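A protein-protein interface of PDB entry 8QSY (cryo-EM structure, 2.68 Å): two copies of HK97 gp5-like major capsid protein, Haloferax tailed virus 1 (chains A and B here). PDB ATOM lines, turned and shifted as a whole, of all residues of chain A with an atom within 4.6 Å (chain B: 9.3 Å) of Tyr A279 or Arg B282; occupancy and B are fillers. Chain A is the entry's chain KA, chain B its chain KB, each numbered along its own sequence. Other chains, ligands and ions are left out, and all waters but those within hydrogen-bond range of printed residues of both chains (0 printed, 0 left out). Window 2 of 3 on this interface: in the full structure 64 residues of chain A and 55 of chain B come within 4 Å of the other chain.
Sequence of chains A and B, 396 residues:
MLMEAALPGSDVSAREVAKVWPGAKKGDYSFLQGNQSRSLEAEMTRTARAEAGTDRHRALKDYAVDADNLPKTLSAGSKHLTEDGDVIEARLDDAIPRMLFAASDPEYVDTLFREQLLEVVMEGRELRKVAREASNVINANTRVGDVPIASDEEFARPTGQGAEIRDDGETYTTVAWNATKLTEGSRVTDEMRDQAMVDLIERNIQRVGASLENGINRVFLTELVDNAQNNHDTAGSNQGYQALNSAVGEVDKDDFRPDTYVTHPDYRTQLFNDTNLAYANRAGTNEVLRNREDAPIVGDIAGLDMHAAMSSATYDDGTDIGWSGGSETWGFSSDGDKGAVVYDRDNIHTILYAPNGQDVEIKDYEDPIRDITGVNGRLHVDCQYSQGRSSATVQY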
ATOM      1  N   THR A 275     -33.912  18.556  -4.024  1.00  0.00           N
ATOM      2  CA  THR A 275     -33.412  19.259  -2.843  1.00  0.00           C
ATOM      3  C   THR A 275     -34.406  19.232  -1.680  1.00  0.00           C
ATOM      4  O   THR A 275     -33.990  19.240  -0.529  1.00  0.00           O
ATOM      5  CB  THR A 275     -32.965  20.695  -3.125  1.00  0.00           C
ATOM      6  OG1 THR A 275     -34.114  21.523  -3.317  1.00  0.00           O
ATOM      7  CG2 THR A 275     -32.019  20.812  -4.296  1.00  0.00           C
ATOM      8  N   ASN A 276     -35.706  19.138  -1.961  1.00  0.00           N
ATOM      9  CA  ASN A 276     -36.733  19.048  -0.934  1.00  0.00           C
ATOM     10  C   ASN A 276     -36.583  17.781  -0.074  1.00  0.00           C
ATOM     11  O   ASN A 276     -37.084  17.764   1.047  1.00  0.00           O
ATOM     12  CB  ASN A 276     -38.111  19.080  -1.599  1.00  0.00           C
ATOM     13  CG  ASN A 276     -39.209  19.708  -0.762  1.00  0.00           C
ATOM     14  OD1 ASN A 276     -40.175  20.228  -1.317  1.00  0.00           O
ATOM     15  ND2 ASN A 276     -39.095  19.677   0.558  1.00  0.00           N
ATOM     16  N   LEU A 277     -35.892  16.743  -0.580  1.00  0.00           N
ATOM     17  CA  LEU A 277     -35.612  15.496   0.125  1.00  0.00           C
ATOM     18  C   LEU A 277     -34.121  15.340   0.439  1.00  0.00           C
ATOM     19  O   LEU A 277     -33.764  14.830   1.501  1.00  0.00           O
ATOM     20  CB  LEU A 277     -36.126  14.320  -0.710  1.00  0.00           C
ATOM     21  CG  LEU A 277     -37.641  14.269  -0.880  1.00  0.00           C
ATOM     22  CD1 LEU A 277     -38.013  13.152  -1.833  1.00  0.00           C
ATOM     23  CD2 LEU A 277     -38.343  14.061   0.454  1.00  0.00           C
ATOM     24  N   ALA A 278     -33.246  15.767  -0.480  1.00  0.00           N
ATOM     25  CA  ALA A 278     -31.803  15.620  -0.367  1.00  0.00           C
ATOM     26  C   ALA A 278     -31.197  16.540   0.699  1.00  0.00           C
ATOM     27  O   ALA A 278     -30.224  16.163   1.338  1.00  0.00           O
ATOM     28  CB  ALA A 278     -31.170  15.842  -1.714  1.00  0.00           C
ATOM     29  N   TYR A 279     -31.744  17.748   0.886  1.00  0.00           N
ATOM     30  CA  TYR A 279     -31.258  18.670   1.904  1.00  0.00           C
ATOM     31  C   TYR A 279     -32.006  18.401   3.209  1.00  0.00           C
ATOM     32  O   TYR A 279     -33.224  18.573   3.264  1.00  0.00           O
ATOM     33  CB  TYR A 279     -31.477  20.127   1.478  1.00  0.00           C
ATOM     34  CG  TYR A 279     -30.766  20.648   0.248  1.00  0.00           C
ATOM     35  CD1 TYR A 279     -29.889  19.865  -0.496  1.00  0.00           C
ATOM     36  CD2 TYR A 279     -30.943  21.969  -0.149  1.00  0.00           C
ATOM     37  CE1 TYR A 279     -29.226  20.372  -1.609  1.00  0.00           C
ATOM     38  CE2 TYR A 279     -30.293  22.489  -1.261  1.00  0.00           C
ATOM     39  CZ  TYR A 279     -29.433  21.687  -1.997  1.00  0.00           C
ATOM     40  OH  TYR A 279     -28.792  22.186  -3.099  1.00  0.00           O
ATOM     41  N   ALA A 280     -31.277  18.055   4.278  1.00  0.00           N
ATOM     42  CA  ALA A 280     -31.874  17.726   5.568  1.00  0.00           C
ATOM     43  C   ALA A 280     -32.724  18.880   6.099  1.00  0.00           C
ATOM     44  O   ALA A 280     -33.832  18.676   6.597  1.00  0.00           O
ATOM     45  CB  ALA A 280     -30.795  17.330   6.536  1.00  0.00           C
ATOM     46  N   ASN A 281     -32.212  20.101   5.930  1.00  0.00           N
ATOM     47  CA  ASN A 281     -32.891  21.377   6.082  1.00  0.00           C
ATOM     48  C   ASN A 281     -34.339  21.347   5.557  1.00  0.00           C
ATOM     49  O   ASN A 281     -35.290  21.618   6.293  1.00  0.00           O
ATOM     50  CB  ASN A 281     -32.032  22.386   5.322  1.00  0.00           C
ATOM     51  CG  ASN A 281     -32.436  23.821   5.534  1.00  0.00           C
ATOM     52  OD1 ASN A 281     -32.883  24.199   6.615  1.00  0.00           O
ATOM     53  ND2 ASN A 281     -32.249  24.632   4.509  1.00  0.00           N
ATOM     54  N   ARG A 282     -34.518  20.998   4.274  1.00  0.00           N
ATOM     55  CA  ARG A 282     -35.804  21.039   3.595  1.00  0.00           C
ATOM     56  C   ARG A 282     -36.663  19.809   3.900  1.00  0.00           C
ATOM     57  O   ARG A 282     -37.882  19.923   3.908  1.00  0.00           O
ATOM     58  CB  ARG A 282     -35.617  21.193   2.083  1.00  0.00           C
ATOM     59  CG  ARG A 282     -34.844  22.426   1.638  1.00  0.00           C
ATOM     60  CD  ARG A 282     -35.077  22.599   0.143  1.00  0.00           C
ATOM     61  NE  ARG A 282     -34.143  23.374  -0.673  1.00  0.00           N
ATOM     62  CZ  ARG A 282     -33.721  24.614  -0.456  1.00  0.00           C
ATOM     63  NH1 ARG A 282     -32.933  25.205  -1.334  1.00  0.00           N
ATOM     64  NH2 ARG A 282     -34.118  25.290   0.610  1.00  0.00           N
ATOM     65  N   ALA A 283     -36.059  18.638   4.133  1.00  0.00           N
ATOM     66  CA  ALA A 283     -36.781  17.394   4.377  1.00  0.00           C
ATOM     67  C   ALA A 283     -37.185  17.198   5.844  1.00  0.00           C
ATOM     68  O   ALA A 283     -38.055  16.376   6.137  1.00  0.00           O
ATOM     69  CB  ALA A 283     -35.930  16.249   3.901  1.00  0.00           C
ATOM     70  N   LEU A 289     -30.662  11.487   2.464  1.00  0.00           N
ATOM     71  CA  LEU A 289     -29.243  11.629   2.161  1.00  0.00           C
ATOM     72  C   LEU A 289     -28.432  10.419   2.649  1.00  0.00           C
ATOM     73  O   LEU A 289     -27.565   9.932   1.928  1.00  0.00           O
ATOM     74  CB  LEU A 289     -28.752  12.948   2.767  1.00  0.00           C
ATOM     75  CG  LEU A 289     -27.245  13.194   2.763  1.00  0.00           C
ATOM     76  CD1 LEU A 289     -26.697  13.261   1.347  1.00  0.00           C
ATOM     77  CD2 LEU A 289     -26.916  14.470   3.515  1.00  0.00           C
ATOM     78  N   TYR B 241     -22.680  14.285  -4.141  1.00  0.00           N
ATOM     79  CA  TYR B 241     -23.709  13.339  -3.731  1.00  0.00           C
ATOM     80  C   TYR B 241     -24.572  12.877  -4.913  1.00  0.00           C
ATOM     81  O   TYR B 241     -24.901  11.695  -5.004  1.00  0.00           O
ATOM     82  CB  TYR B 241     -24.542  13.921  -2.584  1.00  0.00           C
ATOM     83  CG  TYR B 241     -25.905  13.286  -2.463  1.00  0.00           C
ATOM     84  CD1 TYR B 241     -26.073  12.050  -1.847  1.00  0.00           C
ATOM     85  CD2 TYR B 241     -27.022  13.890  -3.027  1.00  0.00           C
ATOM     86  CE1 TYR B 241     -27.321  11.443  -1.779  1.00  0.00           C
ATOM     87  CE2 TYR B 241     -28.269  13.285  -2.984  1.00  0.00           C
ATOM     88  CZ  TYR B 241     -28.424  12.063  -2.347  1.00  0.00           C
ATOM     89  OH  TYR B 241     -29.653  11.461  -2.305  1.00  0.00           O
ATOM     90  N   GLN B 242     -24.899  13.774  -5.852  1.00  0.00           N
ATOM     91  CA  GLN B 242     -25.715  13.408  -7.004  1.00  0.00           C
ATOM     92  C   GLN B 242     -25.081  12.304  -7.859  1.00  0.00           C
ATOM     93  O   GLN B 242     -25.790  11.428  -8.350  1.00  0.00           O
ATOM     94  CB  GLN B 242     -26.084  14.629  -7.836  1.00  0.00           C
ATOM     95  CG  GLN B 242     -27.141  15.509  -7.182  1.00  0.00           C
ATOM     96  CD  GLN B 242     -27.888  16.386  -8.159  1.00  0.00           C
ATOM     97  OE1 GLN B 242     -27.713  16.299  -9.375  1.00  0.00           O
ATOM     98  NE2 GLN B 242     -28.752  17.239  -7.626  1.00  0.00           N
ATOM     99  N   ASN B 273     -16.373  19.361  -0.898  1.00  0.00           N
ATOM    100  CA  ASN B 273     -16.810  20.674  -1.357  1.00  0.00           C
ATOM    101  C   ASN B 273     -18.299  20.700  -1.731  1.00  0.00           C
ATOM    102  O   ASN B 273     -18.835  21.789  -1.940  1.00  0.00           O
ATOM    103  CB  ASN B 273     -15.978  21.151  -2.546  1.00  0.00           C
ATOM    104  CG  ASN B 273     -14.567  21.558  -2.185  1.00  0.00           C
ATOM    105  OD1 ASN B 273     -14.287  21.952  -1.057  1.00  0.00           O
ATOM    106  ND2 ASN B 273     -13.666  21.477  -3.149  1.00  0.00           N
ATOM    107  N   ASP B 274     -18.972  19.541  -1.826  1.00  0.00           N
ATOM    108  CA  ASP B 274     -20.389  19.509  -2.161  1.00  0.00           C
ATOM    109  C   ASP B 274     -21.188  20.220  -1.074  1.00  0.00           C
ATOM    110  O   ASP B 274     -21.182  19.814   0.083  1.00  0.00           O
ATOM    111  CB  ASP B 274     -20.886  18.076  -2.364  1.00  0.00           C
ATOM    112  CG  ASP B 274     -22.347  17.947  -2.763  1.00  0.00           C
ATOM    113  OD1 ASP B 274     -23.083  18.955  -2.749  1.00  0.00           O
ATOM    114  OD2 ASP B 274     -22.734  16.829  -3.121  1.00  0.00           O
ATOM    115  N   THR B 275     -21.910  21.262  -1.485  1.00  0.00           N
ATOM    116  CA  THR B 275     -22.773  22.069  -0.640  1.00  0.00           C
ATOM    117  C   THR B 275     -23.718  21.224   0.219  1.00  0.00           C
ATOM    118  O   THR B 275     -23.995  21.569   1.362  1.00  0.00           O
ATOM    119  CB  THR B 275     -23.564  23.027  -1.527  1.00  0.00           C
ATOM    120  OG1 THR B 275     -22.691  23.633  -2.478  1.00  0.00           O
ATOM    121  CG2 THR B 275     -24.173  24.137  -0.723  1.00  0.00           C
ATOM    122  N   ASN B 276     -24.184  20.082  -0.289  1.00  0.00           N
ATOM    123  CA  ASN B 276     -25.093  19.219   0.450  1.00  0.00           C
ATOM    124  C   ASN B 276     -24.423  18.538   1.653  1.00  0.00           C
ATOM    125  O   ASN B 276     -25.111  18.137   2.587  1.00  0.00           O
ATOM    126  CB  ASN B 276     -25.714  18.191  -0.494  1.00  0.00           C
ATOM    127  CG  ASN B 276     -26.991  17.596   0.063  1.00  0.00           C
ATOM    128  OD1 ASN B 276     -27.636  18.161   0.946  1.00  0.00           O
ATOM    129  ND2 ASN B 276     -27.370  16.436  -0.436  1.00  0.00           N
ATOM    130  N   LEU B 277     -23.086  18.417   1.648  1.00  0.00           N
ATOM    131  CA  LEU B 277     -22.309  17.873   2.757  1.00  0.00           C
ATOM    132  C   LEU B 277     -21.593  18.969   3.550  1.00  0.00           C
ATOM    133  O   LEU B 277     -21.461  18.868   4.768  1.00  0.00           O
ATOM    134  CB  LEU B 277     -21.337  16.822   2.217  1.00  0.00           C
ATOM    135  CG  LEU B 277     -22.003  15.572   1.644  1.00  0.00           C
ATOM    136  CD1 LEU B 277     -20.973  14.693   0.961  1.00  0.00           C
ATOM    137  CD2 LEU B 277     -22.728  14.783   2.725  1.00  0.00           C
ATOM    138  N   ALA B 278     -21.128  20.023   2.871  1.00  0.00           N
ATOM    139  CA  ALA B 278     -20.349  21.095   3.472  1.00  0.00           C
ATOM    140  C   ALA B 278     -21.195  21.989   4.387  1.00  0.00           C
ATOM    141  O   ALA B 278     -20.680  22.476   5.390  1.00  0.00           O
ATOM    142  CB  ALA B 278     -19.689  21.892   2.380  1.00  0.00           C
ATOM    143  N   TYR B 279     -22.466  22.233   4.043  1.00  0.00           N
ATOM    144  CA  TYR B 279     -23.348  23.066   4.851  1.00  0.00           C
ATOM    145  C   TYR B 279     -24.080  22.190   5.870  1.00  0.00           C
ATOM    146  O   TYR B 279     -24.821  21.283   5.489  1.00  0.00           O
ATOM    147  CB  TYR B 279     -24.368  23.776   3.958  1.00  0.00           C
ATOM    148  CG  TYR B 279     -23.875  24.828   2.989  1.00  0.00           C
ATOM    149  CD1 TYR B 279     -22.525  25.132   2.828  1.00  0.00           C
ATOM    150  CD2 TYR B 279     -24.795  25.533   2.219  1.00  0.00           C
ATOM    151  CE1 TYR B 279     -22.106  26.101   1.925  1.00  0.00           C
ATOM    152  CE2 TYR B 279     -24.390  26.506   1.316  1.00  0.00           C
ATOM    153  CZ  TYR B 279     -23.041  26.786   1.163  1.00  0.00           C
ATOM    154  OH  TYR B 279     -22.643  27.740   0.268  1.00  0.00           O
ATOM    155  N   ALA B 280     -23.923  22.503   7.163  1.00  0.00           N
ATOM    156  CA  ALA B 280     -24.401  21.660   8.253  1.00  0.00           C
ATOM    157  C   ALA B 280     -25.912  21.419   8.194  1.00  0.00           C
ATOM    158  O   ALA B 280     -26.364  20.291   8.405  1.00  0.00           O
ATOM    159  CB  ALA B 280     -23.995  22.258   9.569  1.00  0.00           C
ATOM    160  N   ASN B 281     -26.689  22.462   7.898  1.00  0.00           N
ATOM    161  CA  ASN B 281     -28.129  22.359   7.728  1.00  0.00           C
ATOM    162  C   ASN B 281     -28.510  21.427   6.570  1.00  0.00           C
ATOM    163  O   ASN B 281     -29.448  20.644   6.708  1.00  0.00           O
ATOM    164  CB  ASN B 281     -28.750  23.742   7.549  1.00  0.00           C
ATOM    165  CG  ASN B 281     -28.205  24.480   6.344  1.00  0.00           C
ATOM    166  OD1 ASN B 281     -26.995  24.538   6.130  1.00  0.00           O
ATOM    167  ND2 ASN B 281     -29.090  25.004   5.517  1.00  0.00           N
ATOM    168  N   ARG B 282     -27.787  21.474   5.443  1.00  0.00           N
ATOM    169  CA  ARG B 282     -28.079  20.599   4.310  1.00  0.00           C
ATOM    170  C   ARG B 282     -27.715  19.147   4.614  1.00  0.00           C
ATOM    171  O   ARG B 282     -28.502  18.256   4.330  1.00  0.00           O
ATOM    172  CB  ARG B 282     -27.455  21.119   3.017  1.00  0.00           C
ATOM    173  CG  ARG B 282     -27.991  22.497   2.669  1.00  0.00           C
ATOM    174  CD  ARG B 282     -27.660  22.952   1.264  1.00  0.00           C
ATOM    175  NE  ARG B 282     -28.198  24.291   1.052  1.00  0.00           N
ATOM    176  CZ  ARG B 282     -28.069  25.022  -0.051  1.00  0.00           C
ATOM    177  NH1 ARG B 282     -28.613  26.223  -0.106  1.00  0.00           N
ATOM    178  NH2 ARG B 282     -27.398  24.560  -1.091  1.00  0.00           N
ATOM    179  N   ALA B 283     -26.581  18.924   5.284  1.00  0.00           N
ATOM    180  CA  ALA B 283     -26.128  17.601   5.697  1.00  0.00           C
ATOM    181  C   ALA B 283     -26.904  17.028   6.887  1.00  0.00           C
ATOM    182  O   ALA B 283     -26.874  15.819   7.114  1.00  0.00           O
ATOM    183  CB  ALA B 283     -24.675  17.700   6.047  1.00  0.00           C
ATOM    184  N   GLY B 284     -27.530  17.884   7.701  1.00  0.00           N
ATOM    185  CA  GLY B 284     -28.097  17.493   8.988  1.00  0.00           C
ATOM    186  C   GLY B 284     -27.075  17.378  10.127  1.00  0.00           C
ATOM    187  O   GLY B 284     -27.451  17.024  11.244  1.00  0.00           O
ATOM    188  N   THR B 285     -25.792  17.658   9.847  1.00  0.00           N
ATOM    189  CA  THR B 285     -24.690  17.615  10.804  1.00  0.00           C
ATOM    190  C   THR B 285     -23.526  18.467  10.286  1.00  0.00           C
ATOM    191  O   THR B 285     -23.319  18.529   9.085  1.00  0.00           O
ATOM    192  CB  THR B 285     -24.251  16.167  11.082  1.00  0.00           C
ATOM    193  OG1 THR B 285     -23.176  16.218  12.018  1.00  0.00           O
ATOM    194  CG2 THR B 285     -23.769  15.404   9.863  1.00  0.00           C
ATOM    195  N   ASN B 286     -22.720  19.068  11.179  1.00  0.00           N
ATOM    196  CA  ASN B 286     -21.506  19.766  10.768  1.00  0.00           C
ATOM    197  C   ASN B 286     -20.260  18.871  10.715  1.00  0.00           C
ATOM    198  O   ASN B 286     -19.162  19.377  10.478  1.00  0.00           O
ATOM    199  CB  ASN B 286     -21.289  21.061  11.553  1.00  0.00           C
ATOM    200  CG  ASN B 286     -20.891  20.893  13.005  1.00  0.00           C
ATOM    201  OD1 ASN B 286     -20.798  19.787  13.541  1.00  0.00           O
ATOM    202  ND2 ASN B 286     -20.628  22.014  13.656  1.00  0.00           N
ATOM    203  N   VAL B 288     -18.891  16.840   8.465  1.00  0.00           N
ATOM    204  CA  VAL B 288     -18.038  16.887   7.274  1.00  0.00           C
ATOM    205  C   VAL B 288     -17.184  18.154   7.257  1.00  0.00           C
ATOM    206  O   VAL B 288     -15.993  18.088   6.952  1.00  0.00           O
ATOM    207  CB  VAL B 288     -18.824  16.719   5.958  1.00  0.00           C
ATOM    208  CG1 VAL B 288     -17.933  16.821   4.723  1.00  0.00           C
ATOM    209  CG2 VAL B 288     -19.555  15.395   5.955  1.00  0.00           C
ATOM    210  N   ILE B 297     -21.292  10.461   8.649  1.00  0.00           N
ATOM    211  CA  ILE B 297     -22.122  10.571   7.454  1.00  0.00           C
ATOM    212  C   ILE B 297     -21.395  10.140   6.172  1.00  0.00           C
ATOM    213  O   ILE B 297     -22.033   9.651   5.243  1.00  0.00           O
ATOM    214  CB  ILE B 297     -22.762  11.971   7.326  1.00  0.00           C
ATOM    215  CG1 ILE B 297     -23.818  11.999   6.219  1.00  0.00           C
ATOM    216  CG2 ILE B 297     -21.705  13.046   7.120  1.00  0.00           C
ATOM    217  CD1 ILE B 297     -24.904  13.046   6.402  1.00  0.00           C
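OH of Tyr A279 lies within hydrogen-bond range of NH2 of Arg B282 (3.4 Å).
The side-chain amide oxygen of Asn B276 sits close to the backbone carbonyl oxygen of Ala A278, 3.3 Å away.
N of Ala A280 is in hydrogen-bond range of O of Arg B282 (2.8 Å).
The backbone carbonyl oxygen of Asn B281 is in hydrogen-bond range of the backbone NH of Asn A281 (2.9 Å).
OD1 of Asn B276 lies close to O of Arg B282 (3.5 Å).
The backbone NH (N) of Ala B283 sits at hydrogen-bond distance from the backbone carbonyl oxygen (O) of Asn B276.
The backbone NH (N) of Asn B276 is in hydrogen-bond range of the side-chain carboxylate (OD1) of Asp B274, 2.9 Å away.
OD2 of Asp B274 is in hydrogen-bond range of N of Tyr B241, 2.7 Å away.
Among the printed residues, pairs that only touch across the chains: Tyr A279 with Asn B276 (3.2 Å), Ala A280 with Asn B281 (3.6 Å), Ala A280 with Ala B283 (3.9 Å), Ala A280 with Gly B284 (3.5 Å), Leu A289 with Tyr B241 (3.5 Å), Leu A289 with Asn B276 (3.7 Å), Leu A289 with Ala B283 (3.8 Å) and Leu A289 with Ile B297 (3.8 Å).
Of the printed residues of chain B, Ala A278 touches Asn B276 (3.3 Å).
Tyr A279 touches just these residues of chain B: Asn B276 and Arg B282.
Printed residues of chain B within 4 Å of Ala A280: Asn B281 (3.6 Å), Arg B282 (2.8 Å), Ala B283 (3.9 Å) and Gly B284 (3.5 Å).
Of the printed residues of chain B, Asn A281 touches Asn B281 (2.9 Å).
No residue of chain B comes within 4 Å of Arg A282.
Printed residues of chain B within 4 Å of Leu A289: Tyr B241 (3.5 Å), Asn B276 (3.7 Å), Ala B283 (3.8 Å) and Ile B297 (3.8 Å).
Leu B277 touches none of the printed residues of chain A.
Tyr B279 touches none of the printed residues of chain A.
Arg B282 touches just these residues of chain A: Tyr A279 and Ala A280.
Of the printed residues of chain A, Gly B284 touches Ala A280.
Of the printed residues of chain A, Ile B297 touches Leu A289.
The nearest printed residue of chain A that does not touch Ala B283 is Tyr A279 (5.8 Å).
Hydrophobic or aromatic side chains of chain B within 4 Å of the printed part of chain A: Tyr B241 and Ile B297.
Hydrophobic or aromatic side chains of chain A that line the printed part of chain B: Tyr A279, Ala A280 and Leu A289.
Among the printed residues, no Asp or Glu carboxylate lies within 4 Å of a Lys or Arg side-chain nitrogen of the other chain.
Ala A278 touches Asn B276, but with the chains exchanged Asn A276 does not touch Ala B278 (15.4 Å).
Tyr A279 touches Asn B276, but with the chains exchanged Asn A276 does not touch Tyr B279 (13.3 Å).
Tyr A279 touches Arg B282, but with the chains exchanged Arg A282 does not touch Tyr B279 (8.9 Å).
Ala A280 touches Ala B283, but with the chains exchanged Ala A283 does not touch Ala B280 (10.7 Å).
Positions printed for both chains: 275, 276, 277, 278, 279, 280, 281, 282 and 283.
Of the 12 pairs that touch across the chains among the printed residues, 1 has its exchanged pair printed and touching as well.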
